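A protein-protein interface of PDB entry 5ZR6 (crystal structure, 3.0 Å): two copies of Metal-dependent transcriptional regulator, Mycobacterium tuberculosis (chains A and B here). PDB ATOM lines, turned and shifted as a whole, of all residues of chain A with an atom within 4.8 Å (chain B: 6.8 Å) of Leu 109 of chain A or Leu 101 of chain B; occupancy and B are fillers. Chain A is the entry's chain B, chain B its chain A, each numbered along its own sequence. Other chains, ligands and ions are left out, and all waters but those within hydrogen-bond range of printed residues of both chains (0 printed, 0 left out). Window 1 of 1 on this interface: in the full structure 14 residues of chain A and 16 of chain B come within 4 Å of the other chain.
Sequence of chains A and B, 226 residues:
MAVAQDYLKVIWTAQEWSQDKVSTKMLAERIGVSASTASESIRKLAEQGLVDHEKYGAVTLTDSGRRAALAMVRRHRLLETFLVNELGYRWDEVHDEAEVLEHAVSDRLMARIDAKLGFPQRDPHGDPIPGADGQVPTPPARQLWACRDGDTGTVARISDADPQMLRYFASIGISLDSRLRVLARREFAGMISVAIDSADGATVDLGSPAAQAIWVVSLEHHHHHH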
ATOM      1  N   LEU A 101     -27.652 -21.324 -27.990  1.00  0.00           N
ATOM      2  CA  LEU A 101     -27.658 -20.533 -26.760  1.00  0.00           C
ATOM      3  C   LEU A 101     -28.980 -19.811 -26.547  1.00  0.00           C
ATOM      4  O   LEU A 101     -29.359 -19.544 -25.402  1.00  0.00           O
ATOM      5  CB  LEU A 101     -26.521 -19.507 -26.764  1.00  0.00           C
ATOM      6  CG  LEU A 101     -25.093 -19.930 -26.414  1.00  0.00           C
ATOM      7  CD1 LEU A 101     -25.090 -21.085 -25.430  1.00  0.00           C
ATOM      8  CD2 LEU A 101     -24.308 -20.280 -27.657  1.00  0.00           C
ATOM      9  N   ALA A 104     -31.259 -21.040 -23.704  1.00  0.00           N
ATOM     10  CA  ALA A 104     -30.762 -21.184 -22.341  1.00  0.00           C
ATOM     11  C   ALA A 104     -30.090 -19.905 -21.859  1.00  0.00           C
ATOM     12  O   ALA A 104     -29.064 -19.942 -21.178  1.00  0.00           O
ATOM     13  CB  ALA A 104     -29.802 -22.366 -22.235  1.00  0.00           C
ATOM     14  N   VAL A 105     -30.664 -18.754 -22.202  1.00  0.00           N
ATOM     15  CA  VAL A 105     -30.143 -17.459 -21.786  1.00  0.00           C
ATOM     16  C   VAL A 105     -31.252 -16.683 -21.089  1.00  0.00           C
ATOM     17  O   VAL A 105     -32.404 -16.695 -21.533  1.00  0.00           O
ATOM     18  CB  VAL A 105     -29.579 -16.657 -22.977  1.00  0.00           C
ATOM     19  CG1 VAL A 105     -29.279 -15.241 -22.550  1.00  0.00           C
ATOM     20  CG2 VAL A 105     -28.319 -17.312 -23.511  1.00  0.00           C
ATOM     21  N   SER A 106     -30.900 -16.011 -19.999  1.00  0.00           N
ATOM     22  CA  SER A 106     -31.845 -15.208 -19.240  1.00  0.00           C
ATOM     23  C   SER A 106     -31.894 -13.780 -19.776  1.00  0.00           C
ATOM     24  O   SER A 106     -30.955 -13.294 -20.413  1.00  0.00           O
ATOM     25  CB  SER A 106     -31.472 -15.201 -17.756  1.00  0.00           C
ATOM     26  OG  SER A 106     -30.407 -14.301 -17.492  1.00  0.00           O
ATOM     27  N   ASP A 107     -33.016 -13.106 -19.507  1.00  0.00           N
ATOM     28  CA  ASP A 107     -33.161 -11.720 -19.936  1.00  0.00           C
ATOM     29  C   ASP A 107     -32.213 -10.796 -19.179  1.00  0.00           C
ATOM     30  O   ASP A 107     -31.863  -9.723 -19.685  1.00  0.00           O
ATOM     31  CB  ASP A 107     -34.610 -11.261 -19.762  1.00  0.00           C
ATOM     32  CG  ASP A 107     -35.561 -11.935 -20.736  1.00  0.00           C
ATOM     33  OD1 ASP A 107     -35.088 -12.520 -21.736  1.00  0.00           O
ATOM     34  OD2 ASP A 107     -36.786 -11.880 -20.503  1.00  0.00           O
ATOM     35  N   ARG A 108     -31.792 -11.183 -17.974  1.00  0.00           N
ATOM     36  CA  ARG A 108     -30.768 -10.405 -17.284  1.00  0.00           C
ATOM     37  C   ARG A 108     -29.423 -10.542 -17.985  1.00  0.00           C
ATOM     38  O   ARG A 108     -28.687  -9.561 -18.128  1.00  0.00           O
ATOM     39  CB  ARG A 108     -30.662 -10.836 -15.820  1.00  0.00           C
ATOM     40  CG  ARG A 108     -29.313 -10.521 -15.182  1.00  0.00           C
ATOM     41  CD  ARG A 108     -29.144 -11.218 -13.848  1.00  0.00           C
ATOM     42  NE  ARG A 108     -29.599 -10.387 -12.734  1.00  0.00           N
ATOM     43  CZ  ARG A 108     -29.776 -10.828 -11.492  1.00  0.00           C
ATOM     44  NH1 ARG A 108     -29.540 -12.101 -11.193  1.00  0.00           N
ATOM     45  NH2 ARG A 108     -30.191  -9.999 -10.547  1.00  0.00           N
ATOM     46  N   LEU A 109     -29.094 -11.752 -18.441  1.00  0.00           N
ATOM     47  CA  LEU A 109     -27.832 -11.959 -19.140  1.00  0.00           C
ATOM     48  C   LEU A 109     -27.825 -11.241 -20.484  1.00  0.00           C
ATOM     49  O   LEU A 109     -26.803 -10.665 -20.877  1.00  0.00           O
ATOM     50  CB  LEU A 109     -27.577 -13.454 -19.319  1.00  0.00           C
ATOM     51  CG  LEU A 109     -26.476 -13.852 -20.297  1.00  0.00           C
ATOM     52  CD1 LEU A 109     -25.143 -13.372 -19.774  1.00  0.00           C
ATOM     53  CD2 LEU A 109     -26.452 -15.360 -20.476  1.00  0.00           C
ATOM     54  N   MET A 110     -28.954 -11.259 -21.198  1.00  0.00           N
ATOM     55  CA  MET A 110     -29.042 -10.525 -22.456  1.00  0.00           C
ATOM     56  C   MET A 110     -28.825  -9.032 -22.246  1.00  0.00           C
ATOM     57  O   MET A 110     -28.138  -8.382 -23.040  1.00  0.00           O
ATOM     58  CB  MET A 110     -30.391 -10.775 -23.125  1.00  0.00           C
ATOM     59  CG  MET A 110     -30.466 -12.078 -23.889  1.00  0.00           C
ATOM     60  SD  MET A 110     -28.875 -12.468 -24.643  1.00  0.00           S
ATOM     61  CE  MET A 110     -29.333 -13.852 -25.675  1.00  0.00           C
ATOM     62  N   ALA A 111     -29.400  -8.474 -21.177  1.00  0.00           N
ATOM     63  CA  ALA A 111     -29.273  -7.043 -20.932  1.00  0.00           C
ATOM     64  C   ALA A 111     -27.823  -6.646 -20.683  1.00  0.00           C
ATOM     65  O   ALA A 111     -27.388  -5.568 -21.107  1.00  0.00           O
ATOM     66  CB  ALA A 111     -30.157  -6.637 -19.754  1.00  0.00           C
ATOM     67  N   ARG A 112     -27.056  -7.502 -20.004  1.00  0.00           N
ATOM     68  CA  ARG A 112     -25.648  -7.197 -19.763  1.00  0.00           C
ATOM     69  C   ARG A 112     -24.808  -7.426 -21.014  1.00  0.00           C
ATOM     70  O   ARG A 112     -23.857  -6.677 -21.272  1.00  0.00           O
ATOM     71  CB  ARG A 112     -25.120  -8.029 -18.596  1.00  0.00           C
ATOM     72  CG  ARG A 112     -26.068  -8.075 -17.413  1.00  0.00           C
ATOM     73  CD  ARG A 112     -25.333  -8.057 -16.087  1.00  0.00           C
ATOM     74  NE  ARG A 112     -26.117  -7.394 -15.047  1.00  0.00           N
ATOM     75  CZ  ARG A 112     -26.395  -7.935 -13.865  1.00  0.00           C
ATOM     76  NH1 ARG A 112     -25.951  -9.148 -13.570  1.00  0.00           N
ATOM     77  NH2 ARG A 112     -27.119  -7.265 -12.978  1.00  0.00           N
ATOM     78  N   ILE A 113     -25.132  -8.460 -21.794  1.00  0.00           N
ATOM     79  CA  ILE A 113     -24.548  -8.596 -23.126  1.00  0.00           C
ATOM     80  C   ILE A 113     -24.878  -7.368 -23.964  1.00  0.00           C
ATOM     81  O   ILE A 113     -24.003  -6.774 -24.607  1.00  0.00           O
ATOM     82  CB  ILE A 113     -25.046  -9.885 -23.803  1.00  0.00           C
ATOM     83  CG1 ILE A 113     -24.523 -11.121 -23.070  1.00  0.00           C
ATOM     84  CG2 ILE A 113     -24.651  -9.909 -25.277  1.00  0.00           C
ATOM     85  CD1 ILE A 113     -25.008 -12.425 -23.666  1.00  0.00           C
ATOM     86  N   ARG B  75     -17.691 -26.682 -17.300  1.00  0.00           N
ATOM     87  CA  ARG B  75     -18.513 -25.702 -18.004  1.00  0.00           C
ATOM     88  C   ARG B  75     -19.250 -24.799 -17.024  1.00  0.00           C
ATOM     89  O   ARG B  75     -19.256 -23.573 -17.181  1.00  0.00           O
ATOM     90  CB  ARG B  75     -19.502 -26.409 -18.933  1.00  0.00           C
ATOM     91  CG  ARG B  75     -18.900 -27.543 -19.739  1.00  0.00           C
ATOM     92  CD  ARG B  75     -19.060 -27.317 -21.231  1.00  0.00           C
ATOM     93  NE  ARG B  75     -20.382 -27.709 -21.709  1.00  0.00           N
ATOM     94  CZ  ARG B  75     -20.689 -28.932 -22.127  1.00  0.00           C
ATOM     95  NH1 ARG B  75     -21.918 -29.199 -22.548  1.00  0.00           N
ATOM     96  NH2 ARG B  75     -19.768 -29.887 -22.121  1.00  0.00           N
ATOM     97  N   LEU B  79     -18.287 -20.821 -16.608  1.00  0.00           N
ATOM     98  CA  LEU B  79     -19.359 -19.884 -16.926  1.00  0.00           C
ATOM     99  C   LEU B  79     -19.601 -18.910 -15.779  1.00  0.00           C
ATOM    100  O   LEU B  79     -19.771 -17.708 -16.007  1.00  0.00           O
ATOM    101  CB  LEU B  79     -20.637 -20.644 -17.276  1.00  0.00           C
ATOM    102  CG  LEU B  79     -20.694 -21.213 -18.696  1.00  0.00           C
ATOM    103  CD1 LEU B  79     -21.968 -22.014 -18.912  1.00  0.00           C
ATOM    104  CD2 LEU B  79     -20.579 -20.098 -19.728  1.00  0.00           C
ATOM    105  N   LEU B  83     -19.173 -14.836 -16.182  1.00  0.00           N
ATOM    106  CA  LEU B  83     -20.235 -13.881 -15.874  1.00  0.00           C
ATOM    107  C   LEU B  83     -19.758 -12.782 -14.930  1.00  0.00           C
ATOM    108  O   LEU B  83     -20.268 -11.657 -14.986  1.00  0.00           O
ATOM    109  CB  LEU B  83     -21.437 -14.609 -15.271  1.00  0.00           C
ATOM    110  CG  LEU B  83     -22.144 -15.640 -16.155  1.00  0.00           C
ATOM    111  CD1 LEU B  83     -23.161 -16.427 -15.348  1.00  0.00           C
ATOM    112  CD2 LEU B  83     -22.813 -14.959 -17.330  1.00  0.00           C
ATOM    113  N   LEU B  87     -18.882  -9.834 -17.688  1.00  0.00           N
ATOM    114  CA  LEU B  87     -20.245  -9.341 -17.837  1.00  0.00           C
ATOM    115  C   LEU B  87     -20.767  -8.586 -16.623  1.00  0.00           C
ATOM    116  O   LEU B  87     -21.859  -8.012 -16.699  1.00  0.00           O
ATOM    117  CB  LEU B  87     -21.189 -10.507 -18.163  1.00  0.00           C
ATOM    118  CG  LEU B  87     -20.756 -11.307 -19.393  1.00  0.00           C
ATOM    119  CD1 LEU B  87     -21.755 -12.396 -19.708  1.00  0.00           C
ATOM    120  CD2 LEU B  87     -20.584 -10.380 -20.591  1.00  0.00           C
ATOM    121  N   TYR B  89     -21.494  -9.685 -13.371  1.00  0.00           N
ATOM    122  CA  TYR B  89     -22.291 -10.330 -12.340  1.00  0.00           C
ATOM    123  C   TYR B  89     -21.606 -10.219 -10.981  1.00  0.00           C
ATOM    124  O   TYR B  89     -20.394 -10.003 -10.878  1.00  0.00           O
ATOM    125  CB  TYR B  89     -22.519 -11.805 -12.667  1.00  0.00           C
ATOM    126  CG  TYR B  89     -23.657 -12.097 -13.621  1.00  0.00           C
ATOM    127  CD1 TYR B  89     -23.671 -11.577 -14.910  1.00  0.00           C
ATOM    128  CD2 TYR B  89     -24.712 -12.911 -13.231  1.00  0.00           C
ATOM    129  CE1 TYR B  89     -24.713 -11.855 -15.779  1.00  0.00           C
ATOM    130  CE2 TYR B  89     -25.755 -13.193 -14.091  1.00  0.00           C
ATOM    131  CZ  TYR B  89     -25.752 -12.663 -15.360  1.00  0.00           C
ATOM    132  OH  TYR B  89     -26.794 -12.949 -16.209  1.00  0.00           O
ATOM    133  N   ASP B  96     -27.395 -19.553 -10.601  1.00  0.00           N
ATOM    134  CA  ASP B  96     -28.638 -19.860 -11.300  1.00  0.00           C
ATOM    135  C   ASP B  96     -28.496 -19.675 -12.806  1.00  0.00           C
ATOM    136  O   ASP B  96     -29.168 -20.367 -13.580  1.00  0.00           O
ATOM    137  CB  ASP B  96     -29.773 -18.997 -10.752  1.00  0.00           C
ATOM    138  CG  ASP B  96     -29.976 -19.184  -9.261  1.00  0.00           C
ATOM    139  OD1 ASP B  96     -29.631 -20.270  -8.747  1.00  0.00           O
ATOM    140  OD2 ASP B  96     -30.483 -18.250  -8.604  1.00  0.00           O
ATOM    141  N   GLU B  97     -27.624 -18.762 -13.239  1.00  0.00           N
ATOM    142  CA  GLU B  97     -27.424 -18.546 -14.669  1.00  0.00           C
ATOM    143  C   GLU B  97     -26.641 -19.695 -15.294  1.00  0.00           C
ATOM    144  O   GLU B  97     -27.092 -20.309 -16.269  1.00  0.00           O
ATOM    145  CB  GLU B  97     -26.707 -17.217 -14.902  1.00  0.00           C
ATOM    146  CG  GLU B  97     -26.641 -16.803 -16.360  1.00  0.00           C
ATOM    147  CD  GLU B  97     -27.962 -16.274 -16.872  1.00  0.00           C
ATOM    148  OE1 GLU B  97     -28.519 -16.879 -17.814  1.00  0.00           O
ATOM    149  OE2 GLU B  97     -28.443 -15.254 -16.332  1.00  0.00           O
ATOM    150  N   ALA B  98     -25.461 -19.997 -14.747  1.00  0.00           N
ATOM    151  CA  ALA B  98     -24.643 -21.079 -15.282  1.00  0.00           C
ATOM    152  C   ALA B  98     -25.289 -22.447 -15.095  1.00  0.00           C
ATOM    153  O   ALA B  98     -24.887 -23.403 -15.764  1.00  0.00           O
ATOM    154  CB  ALA B  98     -23.260 -21.061 -14.633  1.00  0.00           C
ATOM    155  N   GLU B  99     -26.275 -22.563 -14.202  1.00  0.00           N
ATOM    156  CA  GLU B  99     -26.993 -23.825 -14.057  1.00  0.00           C
ATOM    157  C   GLU B  99     -27.850 -24.120 -15.283  1.00  0.00           C
ATOM    158  O   GLU B  99     -28.127 -25.288 -15.580  1.00  0.00           O
ATOM    159  CB  GLU B  99     -27.852 -23.794 -12.792  1.00  0.00           C
ATOM    160  CG  GLU B  99     -28.588 -25.090 -12.482  1.00  0.00           C
ATOM    161  CD  GLU B  99     -27.648 -26.219 -12.109  1.00  0.00           C
ATOM    162  OE1 GLU B  99     -26.712 -25.982 -11.315  1.00  0.00           O
ATOM    163  OE2 GLU B  99     -27.849 -27.347 -12.604  1.00  0.00           O
ATOM    164  N   VAL B 100     -28.269 -23.085 -16.004  1.00  0.00           N
ATOM    165  CA  VAL B 100     -29.046 -23.248 -17.226  1.00  0.00           C
ATOM    166  C   VAL B 100     -28.160 -23.196 -18.465  1.00  0.00           C
ATOM    167  O   VAL B 100     -28.381 -23.942 -19.419  1.00  0.00           O
ATOM    168  CB  VAL B 100     -30.156 -22.179 -17.293  1.00  0.00           C
ATOM    169  CG1 VAL B 100     -31.098 -22.465 -18.452  1.00  0.00           C
ATOM    170  CG2 VAL B 100     -30.915 -22.123 -15.979  1.00  0.00           C
ATOM    171  N   LEU B 101     -27.150 -22.323 -18.460  1.00  0.00           N
ATOM    172  CA  LEU B 101     -26.248 -22.177 -19.596  1.00  0.00           C
ATOM    173  C   LEU B 101     -25.340 -23.383 -19.803  1.00  0.00           C
ATOM    174  O   LEU B 101     -24.711 -23.484 -20.860  1.00  0.00           O
ATOM    175  CB  LEU B 101     -25.392 -20.921 -19.425  1.00  0.00           C
ATOM    176  CG  LEU B 101     -25.697 -19.737 -20.341  1.00  0.00           C
ATOM    177  CD1 LEU B 101     -24.538 -18.756 -20.328  1.00  0.00           C
ATOM    178  CD2 LEU B 101     -25.960 -20.227 -21.754  1.00  0.00           C
ATOM    179  N   GLU B 102     -25.265 -24.297 -18.834  1.00  0.00           N
ATOM    180  CA  GLU B 102     -24.312 -25.397 -18.914  1.00  0.00           C
ATOM    181  C   GLU B 102     -24.688 -26.437 -19.963  1.00  0.00           C
ATOM    182  O   GLU B 102     -23.802 -27.150 -20.445  1.00  0.00           O
ATOM    183  CB  GLU B 102     -24.177 -26.060 -17.543  1.00  0.00           C
ATOM    184  CG  GLU B 102     -25.490 -26.569 -16.983  1.00  0.00           C
ATOM    185  CD  GLU B 102     -25.392 -26.973 -15.526  1.00  0.00           C
ATOM    186  OE1 GLU B 102     -26.361 -27.561 -15.003  1.00  0.00           O
ATOM    187  OE2 GLU B 102     -24.351 -26.689 -14.898  1.00  0.00           O
ATOM    188  N   HIS B 103     -25.964 -26.545 -20.330  1.00  0.00           N
ATOM    189  CA  HIS B 103     -26.407 -27.565 -21.273  1.00  0.00           C
ATOM    190  C   HIS B 103     -26.548 -27.057 -22.701  1.00  0.00           C
ATOM    191  O   HIS B 103     -27.017 -27.807 -23.562  1.00  0.00           O
ATOM    192  CB  HIS B 103     -27.743 -28.174 -20.827  1.00  0.00           C
ATOM    193  CG  HIS B 103     -27.893 -28.304 -19.344  1.00  0.00           C
ATOM    194  ND1 HIS B 103     -27.441 -29.403 -18.645  1.00  0.00           N
ATOM    195  CD2 HIS B 103     -28.468 -27.488 -18.429  1.00  0.00           C
ATOM    196  CE1 HIS B 103     -27.719 -29.253 -17.364  1.00  0.00           C
ATOM    197  NE2 HIS B 103     -28.344 -28.100 -17.205  1.00  0.00           N
ATOM    198  N   ALA B 104     -26.156 -25.815 -22.981  1.00  0.00           N
ATOM    199  CA  ALA B 104     -26.320 -25.247 -24.313  1.00  0.00           C
ATOM    200  C   ALA B 104     -25.003 -24.777 -24.917  1.00  0.00           C
ATOM    201  O   ALA B 104     -25.006 -24.196 -26.011  1.00  0.00           O
ATOM    202  CB  ALA B 104     -27.319 -24.087 -24.278  1.00  0.00           C
ATOM    203  N   VAL B 105     -23.883 -25.019 -24.255  1.00  0.00           N
ATOM    204  CA  VAL B 105     -22.591 -24.503 -24.689  1.00  0.00           C
ATOM    205  C   VAL B 105     -21.798 -25.605 -25.375  1.00  0.00           C
ATOM    206  O   VAL B 105     -21.749 -26.747 -24.898  1.00  0.00           O
ATOM    207  CB  VAL B 105     -21.807 -23.922 -23.501  1.00  0.00           C
ATOM    208  CG1 VAL B 105     -20.413 -23.592 -23.937  1.00  0.00           C
ATOM    209  CG2 VAL B 105     -22.498 -22.680 -22.971  1.00  0.00           C
ATOM    210  N   LEU B 109     -16.955 -22.855 -27.480  1.00  0.00           N
ATOM    211  CA  LEU B 109     -17.226 -21.642 -26.715  1.00  0.00           C
ATOM    212  C   LEU B 109     -16.454 -21.631 -25.401  1.00  0.00           C
ATOM    213  O   LEU B 109     -15.916 -20.591 -25.001  1.00  0.00           O
ATOM    214  CB  LEU B 109     -18.728 -21.503 -26.467  1.00  0.00           C
ATOM    215  CG  LEU B 109     -19.155 -20.251 -25.702  1.00  0.00           C
ATOM    216  CD1 LEU B 109     -18.944 -19.039 -26.575  1.00  0.00           C
ATOM    217  CD2 LEU B 109     -20.609 -20.335 -25.272  1.00  0.00           C
ATOM    218  N   MET B 110     -16.382 -22.777 -24.716  1.00  0.00           N
ATOM    219  CA  MET B 110     -15.580 -22.852 -23.498  1.00  0.00           C
ATOM    220  C   MET B 110     -14.100 -22.645 -23.783  1.00  0.00           C
ATOM    221  O   MET B 110     -13.370 -22.152 -22.919  1.00  0.00           O
ATOM    222  CB  MET B 110     -15.800 -24.193 -22.794  1.00  0.00           C
ATOM    223  CG  MET B 110     -17.208 -24.399 -22.269  1.00  0.00           C
ATOM    224  SD  MET B 110     -18.034 -22.866 -21.782  1.00  0.00           S
ATOM    225  CE  MET B 110     -17.072 -22.360 -20.366  1.00  0.00           C
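Leu 101 of chain B touches its own counterpart, Leu 101 of chain A. Leu 101 of chain A touches Val 105 of chain B, but with the chains exchanged Val 105 of chain A does not touch Leu 101 of chain B (4.1 Å). Ala 104 of chain B touches its own counterpart, Ala 104 of chain A. Leu 109 of chain A touches Leu 101 of chain B, but with the chains exchanged Leu 101 of chain A does not touch Leu 109 of chain B (4.4 Å). Positions printed for both chains: 101, 104, 105, 109 and 110. Of the 15 pairs that touch across the chains among the printed residues, 4 have their exchanged pair printed and touching as well.
Leu 101 of chain A touches Leu 101 of chain B. Ala 104 of chain B touches Leu 101 of chain A (O to CD1, 3.2 Å). Leu 101 of chain A touches Val 105 of chain B (CD1 to CG2, 3.9 Å). O of Val 100 of chain B touches CB of Ala 104 of chain A (3.5 Å). CD2 of Leu 101 of chain B touches O of Ala 104 of chain A, at 3.2 Å. Arg 108 of chain A touches Tyr 89 of chain B. Leu 83 of chain B touches Leu 109 of chain A. CD1 of Leu 109 of chain A touches CD1 of Leu 87 of chain B, 3.5 Å away. Leu 109 of chain A touches Glu 97 of chain B. CD1 of Leu 101 of chain B touches CD2 of Leu 109 of chain A, at 3.9 Å.
Printed residues of chain A that touch a printed residue of chain B: Leu 101, Ala 104, Ser 106, Arg 108, Leu 109 and Arg 112. Hydrophobic or aromatic side chains of chain B within 4 Å of the printed part of chain A: Leu 83, Leu 87, Tyr 89, Leu 101, Ala 104 and Val 105. Among the printed residues, 15 pairs touch across the chains. Among the printed residues, no Asp or Glu carboxylate lies within 4 Å of a Lys or Arg side-chain nitrogen of the other chain.
Printed residues of chain B within 4 Å of Leu 101 of chain A: Leu 101, Ala 104 and Val 105. Of chain B, only Leu 83 (3.7 Å), Leu 87 (3.5 Å), Tyr 89 (3.2 Å), Glu 97 (3.6 Å) and Leu 101 (3.9 Å) come within 4 Å of Leu 109 of chain A. Leu 101 of chain B touches three residues of chain A. Of the printed residues of chain A, Ala 104 of chain B touches Leu 101 (3.2 Å) and Ala 104 (3.6 Å). The nearest printed residue of chain B that does not touch Arg 112 of chain A is Leu 83 of chain B (6.3 Å).
OE2 of Glu 97 of chain B sits at hydrogen-bond distance from OG of Ser 106 of chain A (2.5 Å). The side-chain hydroxyl (OH) of Tyr 89 of chain B sits close to the backbone NH (N) of Leu 109 of chain A (3.4 Å).
The side-chain hydroxyl (OG) of Ser 106 of chain A sits close to the backbone NH (N) of Arg 108 of chain A. The backbone NH (N) of Leu 109 of chain A sits at hydrogen-bond distance from the side-chain hydroxyl (OG) of Ser 106 of chain A. The backbone carbonyl oxygen (O) of Val 105 of chain B lies within hydrogen-bond range of the guanidinium group (NH1) of Arg 75 of chain B (3.4 Å). The side-chain carboxylate (OE2) of Glu 97 of chain B sits at hydrogen-bond distance from the side-chain hydroxyl (OH) of Tyr 89 of chain B (2.8 Å). The backbone NH (N) of Tyr 89 of chain B sits at hydrogen-bond distance from the backbone carbonyl oxygen (O) of Leu 83 of chain B (2.8 Å).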
